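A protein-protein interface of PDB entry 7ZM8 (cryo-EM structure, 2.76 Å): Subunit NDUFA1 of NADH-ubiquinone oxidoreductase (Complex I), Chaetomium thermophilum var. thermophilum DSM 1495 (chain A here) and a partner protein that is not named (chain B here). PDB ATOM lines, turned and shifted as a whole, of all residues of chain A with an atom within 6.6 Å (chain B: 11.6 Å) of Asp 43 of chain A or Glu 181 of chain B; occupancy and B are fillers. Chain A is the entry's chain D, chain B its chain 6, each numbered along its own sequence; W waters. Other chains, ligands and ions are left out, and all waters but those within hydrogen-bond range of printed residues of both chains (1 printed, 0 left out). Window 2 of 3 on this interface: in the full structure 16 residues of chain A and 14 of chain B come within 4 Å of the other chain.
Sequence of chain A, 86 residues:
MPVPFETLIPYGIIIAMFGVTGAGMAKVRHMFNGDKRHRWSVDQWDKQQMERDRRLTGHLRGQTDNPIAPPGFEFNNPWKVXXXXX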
ATOM      1  N   TRP A  40      -7.912  11.196 -35.784  1.00  0.00           N
ATOM      2  CA  TRP A  40      -9.282  11.787 -35.761  1.00  0.00           C
ATOM      3  C   TRP A  40     -10.222  11.193 -34.707  1.00  0.00           C
ATOM      4  O   TRP A  40     -10.232  11.746 -33.608  1.00  0.00           O
ATOM      5  CB  TRP A  40      -9.927  12.092 -37.130  1.00  0.00           C
ATOM      6  CG  TRP A  40     -10.004  11.029 -38.180  1.00  0.00           C
ATOM      7  CD1 TRP A  40     -11.064  10.216 -38.449  1.00  0.00           C
ATOM      8  CD2 TRP A  40      -9.021  10.751 -39.192  1.00  0.00           C
ATOM      9  NE1 TRP A  40     -10.789   9.411 -39.519  1.00  0.00           N
ATOM     10  CE2 TRP A  40      -9.543   9.714 -39.996  1.00  0.00           C
ATOM     11  CE3 TRP A  40      -7.743  11.244 -39.471  1.00  0.00           C
ATOM     12  CZ2 TRP A  40      -8.831   9.169 -41.061  1.00  0.00           C
ATOM     13  CZ3 TRP A  40      -7.042  10.705 -40.524  1.00  0.00           C
ATOM     14  CH2 TRP A  40      -7.580   9.681 -41.306  1.00  0.00           C
ATOM     15  N   SER A  41     -11.037  10.204 -35.014  1.00  0.00           N
ATOM     16  CA  SER A  41     -12.064   9.723 -34.052  1.00  0.00           C
ATOM     17  C   SER A  41     -11.412   9.020 -32.858  1.00  0.00           C
ATOM     18  O   SER A  41     -11.587   7.800 -32.723  1.00  0.00           O
ATOM     19  CB  SER A  41     -13.101   8.899 -34.753  1.00  0.00           C
ATOM     20  OG  SER A  41     -13.797   9.689 -35.704  1.00  0.00           O
ATOM     21  N   VAL A  42     -10.759   9.787 -31.993  1.00  0.00           N
ATOM     22  CA  VAL A  42      -9.955   9.182 -30.904  1.00  0.00           C
ATOM     23  C   VAL A  42     -10.796   8.891 -29.657  1.00  0.00           C
ATOM     24  O   VAL A  42     -11.677   9.698 -29.317  1.00  0.00           O
ATOM     25  CB  VAL A  42      -8.718  10.053 -30.615  1.00  0.00           C
ATOM     26  CG1 VAL A  42      -7.791  10.119 -31.815  1.00  0.00           C
ATOM     27  CG2 VAL A  42      -9.099  11.447 -30.151  1.00  0.00           C
ATOM     28  N   ASP A  43     -10.527   7.765 -28.995  1.00  0.00           N
ATOM     29  CA  ASP A  43     -11.285   7.373 -27.789  1.00  0.00           C
ATOM     30  C   ASP A  43     -10.317   7.260 -26.623  1.00  0.00           C
ATOM     31  O   ASP A  43      -9.171   7.619 -26.809  1.00  0.00           O
ATOM     32  CB  ASP A  43     -12.177   6.164 -28.054  1.00  0.00           C
ATOM     33  CG  ASP A  43     -11.472   4.903 -28.527  1.00  0.00           C
ATOM     34  OD1 ASP A  43     -10.263   4.955 -28.775  1.00  0.00           O
ATOM     35  OD2 ASP A  43     -12.152   3.869 -28.633  1.00  0.00           O
ATOM     36  N   GLN A  44     -10.771   6.724 -25.496  1.00  0.00           N
ATOM     37  CA  GLN A  44      -9.923   6.566 -24.297  1.00  0.00           C
ATOM     38  C   GLN A  44      -8.752   5.683 -24.703  1.00  0.00           C
ATOM     39  O   GLN A  44      -7.638   6.028 -24.340  1.00  0.00           O
ATOM     40  CB  GLN A  44     -10.777   5.938 -23.199  1.00  0.00           C
ATOM     41  CG  GLN A  44     -10.026   5.630 -21.918  1.00  0.00           C
ATOM     42  CD  GLN A  44     -10.826   4.716 -21.024  1.00  0.00           C
ATOM     43  OE1 GLN A  44     -12.014   4.492 -21.242  1.00  0.00           O
ATOM     44  NE2 GLN A  44     -10.173   4.172 -20.010  1.00  0.00           N
ATOM     45  N   TRP A  45      -9.003   4.635 -25.478  1.00  0.00           N
ATOM     46  CA  TRP A  45      -7.940   3.699 -25.908  1.00  0.00           C
ATOM     47  C   TRP A  45      -6.861   4.432 -26.691  1.00  0.00           C
ATOM     48  O   TRP A  45      -5.703   4.289 -26.327  1.00  0.00           O
ATOM     49  CB  TRP A  45      -8.533   2.556 -26.741  1.00  0.00           C
ATOM     50  CG  TRP A  45      -7.546   1.550 -27.244  1.00  0.00           C
ATOM     51  CD1 TRP A  45      -6.689   1.685 -28.296  1.00  0.00           C
ATOM     52  CD2 TRP A  45      -7.335   0.228 -26.726  1.00  0.00           C
ATOM     53  NE1 TRP A  45      -5.942   0.551 -28.450  1.00  0.00           N
ATOM     54  CE2 TRP A  45      -6.314  -0.360 -27.500  1.00  0.00           C
ATOM     55  CE3 TRP A  45      -7.899  -0.510 -25.680  1.00  0.00           C
ATOM     56  CZ2 TRP A  45      -5.851  -1.651 -27.265  1.00  0.00           C
ATOM     57  CZ3 TRP A  45      -7.433  -1.782 -25.443  1.00  0.00           C
ATOM     58  CH2 TRP A  45      -6.422  -2.340 -26.223  1.00  0.00           C
ATOM     59  N   ASP A  46      -7.240   5.137 -27.743  1.00  0.00           N
ATOM     60  CA  ASP A  46      -6.287   5.834 -28.637  1.00  0.00           C
ATOM     61  C   ASP A  46      -5.473   6.835 -27.842  1.00  0.00           C
ATOM     62  O   ASP A  46      -4.266   6.912 -28.074  1.00  0.00           O
ATOM     63  CB  ASP A  46      -7.042   6.551 -29.751  1.00  0.00           C
ATOM     64  CG  ASP A  46      -7.821   5.632 -30.669  1.00  0.00           C
ATOM     65  OD1 ASP A  46      -7.344   4.516 -30.925  1.00  0.00           O
ATOM     66  OD2 ASP A  46      -8.900   6.043 -31.119  1.00  0.00           O
ATOM     67  N   LYS A  47      -6.134   7.615 -27.001  1.00  0.00           N
ATOM     68  CA  LYS A  47      -5.471   8.649 -26.177  1.00  0.00           C
ATOM     69  C   LYS A  47      -4.459   8.014 -25.227  1.00  0.00           C
ATOM     70  O   LYS A  47      -3.426   8.624 -24.988  1.00  0.00           O
ATOM     71  CB  LYS A  47      -6.550   9.410 -25.413  1.00  0.00           C
ATOM     72  CG  LYS A  47      -7.523  10.217 -26.262  1.00  0.00           C
ATOM     73  CD  LYS A  47      -8.599  10.868 -25.426  1.00  0.00           C
ATOM     74  CE  LYS A  47      -9.545  11.747 -26.216  1.00  0.00           C
ATOM     75  NZ  LYS A  47     -10.627  10.966 -26.860  1.00  0.00           N
ATOM     76  N   GLN A  48      -4.782   6.843 -24.680  1.00  0.00           N
ATOM     77  CA  GLN A  48      -3.867   6.128 -23.761  1.00  0.00           C
ATOM     78  C   GLN A  48      -2.738   5.507 -24.578  1.00  0.00           C
ATOM     79  O   GLN A  48      -1.607   5.480 -24.081  1.00  0.00           O
ATOM     80  CB  GLN A  48      -4.650   5.057 -23.004  1.00  0.00           C
ATOM     81  CG  GLN A  48      -5.634   5.608 -21.987  1.00  0.00           C
ATOM     82  CD  GLN A  48      -6.396   4.500 -21.308  1.00  0.00           C
ATOM     83  OE1 GLN A  48      -7.190   4.735 -20.404  1.00  0.00           O
ATOM     84  NE2 GLN A  48      -6.152   3.278 -21.742  1.00  0.00           N
ATOM     85  N   MET A  50      -1.450   6.770 -27.266  1.00  0.00           N
ATOM     86  CA  MET A  50      -0.544   7.904 -27.592  1.00  0.00           C
ATOM     87  C   MET A  50       0.232   8.356 -26.357  1.00  0.00           C
ATOM     88  O   MET A  50       1.365   8.813 -26.533  1.00  0.00           O
ATOM     89  CB  MET A  50      -1.336   9.088 -28.143  1.00  0.00           C
ATOM     90  CG  MET A  50      -1.663   8.953 -29.614  1.00  0.00           C
ATOM     91  SD  MET A  50      -2.485  10.414 -30.283  1.00  0.00           S
ATOM     92  CE  MET A  50      -4.163  10.134 -29.721  1.00  0.00           C
ATOM     93  N   THR B  15      -1.608  17.241 -22.847  1.00  0.00           N
ATOM     94  CA  THR B  15      -2.834  16.557 -22.372  1.00  0.00           C
ATOM     95  C   THR B  15      -3.191  17.236 -21.054  1.00  0.00           C
ATOM     96  O   THR B  15      -3.629  16.528 -20.145  1.00  0.00           O
ATOM     97  CB  THR B  15      -2.525  15.067 -22.219  1.00  0.00           C
ATOM     98  OG1 THR B  15      -1.378  14.960 -21.377  1.00  0.00           O
ATOM     99  CG2 THR B  15      -2.237  14.387 -23.540  1.00  0.00           C
ATOM    100  N   GLY B  65     -17.409  17.593 -18.250  1.00  0.00           N
ATOM    101  CA  GLY B  65     -17.516  16.390 -19.044  1.00  0.00           C
ATOM    102  C   GLY B  65     -18.913  15.872 -19.294  1.00  0.00           C
ATOM    103  O   GLY B  65     -19.052  14.800 -19.890  1.00  0.00           O
ATOM    104  N   LEU B  66     -19.945  16.581 -18.859  1.00  0.00           N
ATOM    105  CA  LEU B  66     -21.323  16.131 -19.052  1.00  0.00           C
ATOM    106  C   LEU B  66     -21.929  16.823 -20.270  1.00  0.00           C
ATOM    107  O   LEU B  66     -22.855  17.624 -20.181  1.00  0.00           O
ATOM    108  CB  LEU B  66     -22.139  16.381 -17.791  1.00  0.00           C
ATOM    109  CG  LEU B  66     -22.132  15.236 -16.786  1.00  0.00           C
ATOM    110  CD1 LEU B  66     -20.811  15.198 -16.094  1.00  0.00           C
ATOM    111  CD2 LEU B  66     -23.232  15.416 -15.772  1.00  0.00           C
ATOM    112  N   ASN B  67     -21.380  16.468 -21.433  1.00  0.00           N
ATOM    113  CA  ASN B  67     -21.701  17.176 -22.668  1.00  0.00           C
ATOM    114  C   ASN B  67     -23.164  17.006 -23.053  1.00  0.00           C
ATOM    115  O   ASN B  67     -23.842  17.982 -23.390  1.00  0.00           O
ATOM    116  CB  ASN B  67     -20.793  16.687 -23.793  1.00  0.00           C
ATOM    117  CG  ASN B  67     -19.345  17.041 -23.559  1.00  0.00           C
ATOM    118  OD1 ASN B  67     -18.974  17.482 -22.475  1.00  0.00           O
ATOM    119  ND2 ASN B  67     -18.516  16.849 -24.578  1.00  0.00           N
ATOM    120  N   PHE B  68     -23.693  15.791 -23.054  1.00  0.00           N
ATOM    121  CA  PHE B  68     -25.045  15.615 -23.639  1.00  0.00           C
ATOM    122  C   PHE B  68     -26.087  16.279 -22.743  1.00  0.00           C
ATOM    123  O   PHE B  68     -26.948  16.964 -23.285  1.00  0.00           O
ATOM    124  CB  PHE B  68     -25.384  14.123 -23.710  1.00  0.00           C
ATOM    125  CG  PHE B  68     -26.829  13.786 -23.968  1.00  0.00           C
ATOM    126  CD1 PHE B  68     -27.442  14.144 -25.158  1.00  0.00           C
ATOM    127  CD2 PHE B  68     -27.569  13.084 -23.032  1.00  0.00           C
ATOM    128  CE1 PHE B  68     -28.770  13.827 -25.393  1.00  0.00           C
ATOM    129  CE2 PHE B  68     -28.895  12.767 -23.270  1.00  0.00           C
ATOM    130  CZ  PHE B  68     -29.493  13.138 -24.448  1.00  0.00           C
ATOM    131  N   LYS B 173      -4.678   4.973 -15.946  1.00  0.00           N
ATOM    132  CA  LYS B 173      -5.307   4.420 -17.174  1.00  0.00           C
ATOM    133  C   LYS B 173      -5.705   2.950 -17.004  1.00  0.00           C
ATOM    134  O   LYS B 173      -5.076   2.276 -16.186  1.00  0.00           O
ATOM    135  CB  LYS B 173      -4.296   4.612 -18.309  1.00  0.00           C
ATOM    136  CG  LYS B 173      -3.133   3.639 -18.375  1.00  0.00           C
ATOM    137  CD  LYS B 173      -2.333   3.786 -19.650  1.00  0.00           C
ATOM    138  CE  LYS B 173      -2.126   5.228 -20.063  1.00  0.00           C
ATOM    139  NZ  LYS B 173      -1.066   5.375 -21.089  1.00  0.00           N
ATOM    140  N   ILE B 174      -6.709   2.468 -17.743  1.00  0.00           N
ATOM    141  CA  ILE B 174      -7.123   1.028 -17.726  1.00  0.00           C
ATOM    142  C   ILE B 174      -7.246   0.564 -19.175  1.00  0.00           C
ATOM    143  O   ILE B 174      -7.492   1.408 -20.027  1.00  0.00           O
ATOM    144  CB  ILE B 174      -8.446   0.795 -16.957  1.00  0.00           C
ATOM    145  CG1 ILE B 174      -8.713  -0.683 -16.679  1.00  0.00           C
ATOM    146  CG2 ILE B 174      -9.625   1.453 -17.653  1.00  0.00           C
ATOM    147  CD1 ILE B 174      -9.943  -0.909 -15.839  1.00  0.00           C
ATOM    148  N   TRP B 175      -7.125  -0.736 -19.437  1.00  0.00           N
ATOM    149  CA  TRP B 175      -7.135  -1.218 -20.840  1.00  0.00           C
ATOM    150  C   TRP B 175      -8.358  -2.090 -21.118  1.00  0.00           C
ATOM    151  O   TRP B 175      -8.994  -1.894 -22.163  1.00  0.00           O
ATOM    152  CB  TRP B 175      -5.819  -1.928 -21.159  1.00  0.00           C
ATOM    153  CG  TRP B 175      -4.665  -0.975 -21.175  1.00  0.00           C
ATOM    154  CD1 TRP B 175      -3.739  -0.784 -20.193  1.00  0.00           C
ATOM    155  CD2 TRP B 175      -4.341  -0.041 -22.218  1.00  0.00           C
ATOM    156  NE1 TRP B 175      -2.847   0.183 -20.564  1.00  0.00           N
ATOM    157  CE2 TRP B 175      -3.192   0.661 -21.799  1.00  0.00           C
ATOM    158  CE3 TRP B 175      -4.901   0.263 -23.465  1.00  0.00           C
ATOM    159  CZ2 TRP B 175      -2.593   1.642 -22.585  1.00  0.00           C
ATOM    160  CZ3 TRP B 175      -4.308   1.231 -24.239  1.00  0.00           C
ATOM    161  CH2 TRP B 175      -3.169   1.907 -23.805  1.00  0.00           C
ATOM    162  N   ASP B 176      -8.662  -3.023 -20.222  1.00  0.00           N
ATOM    163  CA  ASP B 176      -9.844  -3.908 -20.390  1.00  0.00           C
ATOM    164  C   ASP B 176     -11.134  -3.077 -20.359  1.00  0.00           C
ATOM    165  O   ASP B 176     -12.062  -3.421 -21.112  1.00  0.00           O
ATOM    166  CB  ASP B 176      -9.780  -5.144 -19.481  1.00  0.00           C
ATOM    167  CG  ASP B 176      -9.344  -4.887 -18.050  1.00  0.00           C
ATOM    168  OD1 ASP B 176      -9.350  -3.717 -17.631  1.00  0.00           O
ATOM    169  OD2 ASP B 176      -9.006  -5.868 -17.363  1.00  0.00           O
ATOM    170  N   GLY B 177     -11.195  -2.045 -19.518  1.00  0.00           N
ATOM    171  CA  GLY B 177     -12.382  -1.175 -19.432  1.00  0.00           C
ATOM    172  C   GLY B 177     -12.382  -0.053 -20.458  1.00  0.00           C
ATOM    173  O   GLY B 177     -13.296   0.782 -20.399  1.00  0.00           O
ATOM    174  N   ALA B 178     -11.397  -0.014 -21.357  1.00  0.00           N
ATOM    175  CA  ALA B 178     -11.352   0.986 -22.445  1.00  0.00           C
ATOM    176  C   ALA B 178     -11.574   0.347 -23.810  1.00  0.00           C
ATOM    177  O   ALA B 178     -11.434   1.089 -24.783  1.00  0.00           O
ATOM    178  CB  ALA B 178     -10.010   1.668 -22.418  1.00  0.00           C
ATOM    179  N   LEU B 179     -11.882  -0.949 -23.907  1.00  0.00           N
ATOM    180  CA  LEU B 179     -11.956  -1.629 -25.236  1.00  0.00           C
ATOM    181  C   LEU B 179     -12.887  -0.891 -26.195  1.00  0.00           C
ATOM    182  O   LEU B 179     -12.462  -0.602 -27.304  1.00  0.00           O
ATOM    183  CB  LEU B 179     -12.416  -3.078 -25.063  1.00  0.00           C
ATOM    184  CG  LEU B 179     -12.704  -3.864 -26.342  1.00  0.00           C
ATOM    185  CD1 LEU B 179     -11.422  -4.185 -27.089  1.00  0.00           C
ATOM    186  CD2 LEU B 179     -13.457  -5.146 -26.028  1.00  0.00           C
ATOM    187  N   ALA B 180     -14.103  -0.589 -25.759  1.00  0.00           N
ATOM    188  CA  ALA B 180     -15.102   0.068 -26.611  1.00  0.00           C
ATOM    189  C   ALA B 180     -15.791   1.140 -25.788  1.00  0.00           C
ATOM    190  O   ALA B 180     -16.983   1.008 -25.559  1.00  0.00           O
ATOM    191  CB  ALA B 180     -16.084  -0.977 -27.035  1.00  0.00           C
ATOM    192  N   GLU B 181     -15.084   2.183 -25.393  1.00  0.00           N
ATOM    193  CA  GLU B 181     -15.695   3.192 -24.499  1.00  0.00           C
ATOM    194  C   GLU B 181     -16.846   3.897 -25.211  1.00  0.00           C
ATOM    195  O   GLU B 181     -16.731   4.193 -26.414  1.00  0.00           O
ATOM    196  CB  GLU B 181     -14.650   4.136 -23.900  1.00  0.00           C
ATOM    197  CG  GLU B 181     -15.199   5.415 -23.300  1.00  0.00           C
ATOM    198  CD  GLU B 181     -15.106   6.631 -24.209  1.00  0.00           C
ATOM    199  OE1 GLU B 181     -14.450   6.527 -25.262  1.00  0.00           O
ATOM    200  OE2 GLU B 181     -15.695   7.674 -23.868  1.00  0.00           O
ATOM    201  N   ASN B 182     -17.913   4.177 -24.469  1.00  0.00           N
ATOM    202  CA  ASN B 182     -19.099   4.805 -25.075  1.00  0.00           C
ATOM    203  C   ASN B 182     -19.192   6.235 -24.592  1.00  0.00           C
ATOM    204  O   ASN B 182     -18.656   6.521 -23.520  1.00  0.00           O
ATOM    205  CB  ASN B 182     -20.407   4.108 -24.698  1.00  0.00           C
ATOM    206  CG  ASN B 182     -20.493   2.660 -25.116  1.00  0.00           C
ATOM    207  OD1 ASN B 182     -19.611   2.142 -25.789  1.00  0.00           O
ATOM    208  ND2 ASN B 182     -21.560   2.001 -24.711  1.00  0.00           N
ATOM    209  N   ASN B 183     -19.773   7.103 -25.414  1.00  0.00           N
ATOM    210  CA  ASN B 183     -20.071   8.471 -24.946  1.00  0.00           C
ATOM    211  C   ASN B 183     -21.228   8.317 -23.965  1.00  0.00           C
ATOM    212  O   ASN B 183     -21.924   7.314 -24.054  1.00  0.00           O
ATOM    213  CB  ASN B 183     -20.462   9.355 -26.118  1.00  0.00           C
ATOM    214  CG  ASN B 183     -19.384   9.454 -27.174  1.00  0.00           C
ATOM    215  OD1 ASN B 183     -18.200   9.514 -26.853  1.00  0.00           O
ATOM    216  ND2 ASN B 183     -19.786   9.482 -28.433  1.00  0.00           N
ATOM    217  N   HIS B 184     -21.454   9.281 -23.092  1.00  0.00           N
ATOM    218  CA  HIS B 184     -22.518   9.128 -22.068  1.00  0.00           C
ATOM    219  C   HIS B 184     -23.882   8.881 -22.709  1.00  0.00           C
ATOM    220  O   HIS B 184     -24.624   8.102 -22.135  1.00  0.00           O
ATOM    221  CB  HIS B 184     -22.605  10.338 -21.141  1.00  0.00           C
ATOM    222  CG  HIS B 184     -21.372  10.627 -20.354  1.00  0.00           C
ATOM    223  ND1 HIS B 184     -21.076  11.889 -19.889  1.00  0.00           N
ATOM    224  CD2 HIS B 184     -20.371   9.831 -19.937  1.00  0.00           C
ATOM    225  CE1 HIS B 184     -19.947  11.857 -19.220  1.00  0.00           C
ATOM    226  NE2 HIS B 184     -19.494  10.610 -19.237  1.00  0.00           N
ATOM    227  N   ILE B 185     -24.200   9.527 -23.830  1.00  0.00           N
ATOM    228  CA  ILE B 185     -25.515   9.381 -24.511  1.00  0.00           C
ATOM    229  C   ILE B 185     -25.680   7.925 -24.961  1.00  0.00           C
ATOM    230  O   ILE B 185     -26.788   7.402 -24.870  1.00  0.00           O
ATOM    231  CB  ILE B 185     -25.609  10.407 -25.661  1.00  0.00           C
ATOM    232  CG1 ILE B 185     -26.962  10.341 -26.373  1.00  0.00           C
ATOM    233  CG2 ILE B 185     -24.441  10.287 -26.625  1.00  0.00           C
ATOM    234  CD1 ILE B 185     -27.107  11.290 -27.528  1.00  0.00           C
ATOM    235  N   SER B 186     -24.623   7.316 -25.484  1.00  0.00           N
ATOM    236  CA  SER B 186     -24.647   5.900 -25.899  1.00  0.00           C
ATOM    237  C   SER B 186     -24.857   5.008 -24.678  1.00  0.00           C
ATOM    238  O   SER B 186     -25.626   4.073 -24.786  1.00  0.00           O
ATOM    239  CB  SER B 186     -23.390   5.627 -26.619  1.00  0.00           C
ATOM    240  OG  SER B 186     -23.188   6.595 -27.632  1.00  0.00           O
ATOM    241  N   SER B 187     -24.204   5.316 -23.565  1.00  0.00           N
ATOM    242  CA  SER B 187     -24.414   4.590 -22.293  1.00  0.00           C
ATOM    243  C   SER B 187     -25.838   4.784 -21.745  1.00  0.00           C
ATOM    244  O   SER B 187     -26.399   3.800 -21.253  1.00  0.00           O
ATOM    245  CB  SER B 187     -23.359   5.023 -21.329  1.00  0.00           C
ATOM    246  OG  SER B 187     -22.110   5.143 -21.979  1.00  0.00           O
ATOM    247  N   ILE B 188     -26.386   5.999 -21.794  1.00  0.00           N
ATOM    248  CA  ILE B 188     -27.783   6.276 -21.355  1.00  0.00           C
ATOM    249  C   ILE B 188     -28.696   5.507 -22.288  1.00  0.00           C
ATOM    250  O   ILE B 188     -29.598   4.859 -21.798  1.00  0.00           O
ATOM    251  CB  ILE B 188     -28.082   7.791 -21.373  1.00  0.00           C
ATOM    252  CG1 ILE B 188     -27.292   8.533 -20.293  1.00  0.00           C
ATOM    253  CG2 ILE B 188     -29.573   8.052 -21.241  1.00  0.00           C
ATOM    254  CD1 ILE B 188     -27.382  10.033 -20.384  1.00  0.00           C
ATOM    255  N   ASN B 190     -28.033   2.747 -23.983  1.00  0.00           N
ATOM    256  CA  ASN B 190     -27.908   1.291 -23.757  1.00  0.00           C
ATOM    257  C   ASN B 190     -28.917   0.842 -22.704  1.00  0.00           C
ATOM    258  O   ASN B 190     -29.391  -0.284 -22.817  1.00  0.00           O
ATOM    259  CB  ASN B 190     -26.502   0.888 -23.322  1.00  0.00           C
ATOM    260  CG  ASN B 190     -25.434   1.012 -24.385  1.00  0.00           C
ATOM    261  OD1 ASN B 190     -25.725   1.225 -25.557  1.00  0.00           O
ATOM    262  ND2 ASN B 190     -24.186   0.881 -23.976  1.00  0.00           N
HETATM  263  O   HOH W   1     -12.146   3.316 -25.964  1.00  0.00           O
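Of the 10 printed residues of chain A, 4 touch a printed residue of chain B. Along chain B the printed residues that touch a printed residue of chain A span positions 173 to 181. Among the printed residues, no Asp or Glu carboxylate lies within 4 Å of a Lys or Arg side-chain nitrogen of the other chain.
Among the printed residues, merely in contact across the chains: Asp 43 of chain A with Glu 181 of chain B (3.6 Å), Gln 44 of chain A with Ile 174 of chain B (3.6 Å), Gln 44 of chain A with Ala 178 of chain B (3.4 Å), Gln 44 of chain A with Glu 181 of chain B (3.7 Å), Trp 45 of chain A with Trp 175 of chain B (3.6 Å), Trp 45 of chain A with Ala 178 of chain B (3.8 Å) and Gln 48 of chain A with Trp 175 of chain B (3.6 Å).
The backbone NH (N) of Asp 43 of chain A sits at hydrogen-bond distance from the side-chain carboxylate (OD2) of Asp 46 of chain A, 3.2 Å away. The side-chain amide oxygen (OE1) of Gln 48 of chain A lies within hydrogen-bond range of the side-chain amide nitrogen (NE2) of Gln 44 of chain A, 3.1 Å away.
The side-chain amino group (NZ) of Lys 173 of chain B is in hydrogen-bond range of the backbone carbonyl oxygen (O) of Gln 48 of chain A. O of Ile 174 of chain B is in hydrogen-bond range of NE2 of Gln 48 of chain A (2.9 Å).
No residue of chain B comes within 4 Å of Val 42 of chain A. Of chain B, only Glu 181 (3.6 Å) comes within 4 Å of Asp 43 of chain A. Of the printed residues of chain B, Gln 44 of chain A touches Ile 174 (3.6 Å), Ala 178 (3.4 Å) and Glu 181 (3.7 Å). No residue of chain B comes within 4 Å of Asp 46 of chain A. Of the printed residues of chain B, Gln 48 of chain A touches Lys 173 (3.0 Å), Ile 174 (2.9 Å) and Trp 175 (3.6 Å). Of the printed residues of chain A, Lys 173 of chain B touches Gln 48 (3.0 Å). Of the printed residues of chain A, Ala 178 of chain B touches Gln 44 and Trp 45. Of the printed residues of chain A, Glu 181 of chain B touches Asp 43 and Gln 44. Asn 190 of chain B touches none of the printed residues of chain A. The nearest residue of chain B that does not touch Asp 43 of chain A is Leu 179 of chain B (4.7 Å). The nearest residue of chain A that does not touch Glu 181 of chain B is Trp 45 of chain A (5.8 Å).
Water W1 lies within hydrogen-bond range of O of Ala 178 of chain B (2.6 Å), OD2 of Asp 43 of chain A (2.7 Å), N of Glu 181 of chain B (3.2 Å) and N of Trp 45 of chain A (3.4 Å).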
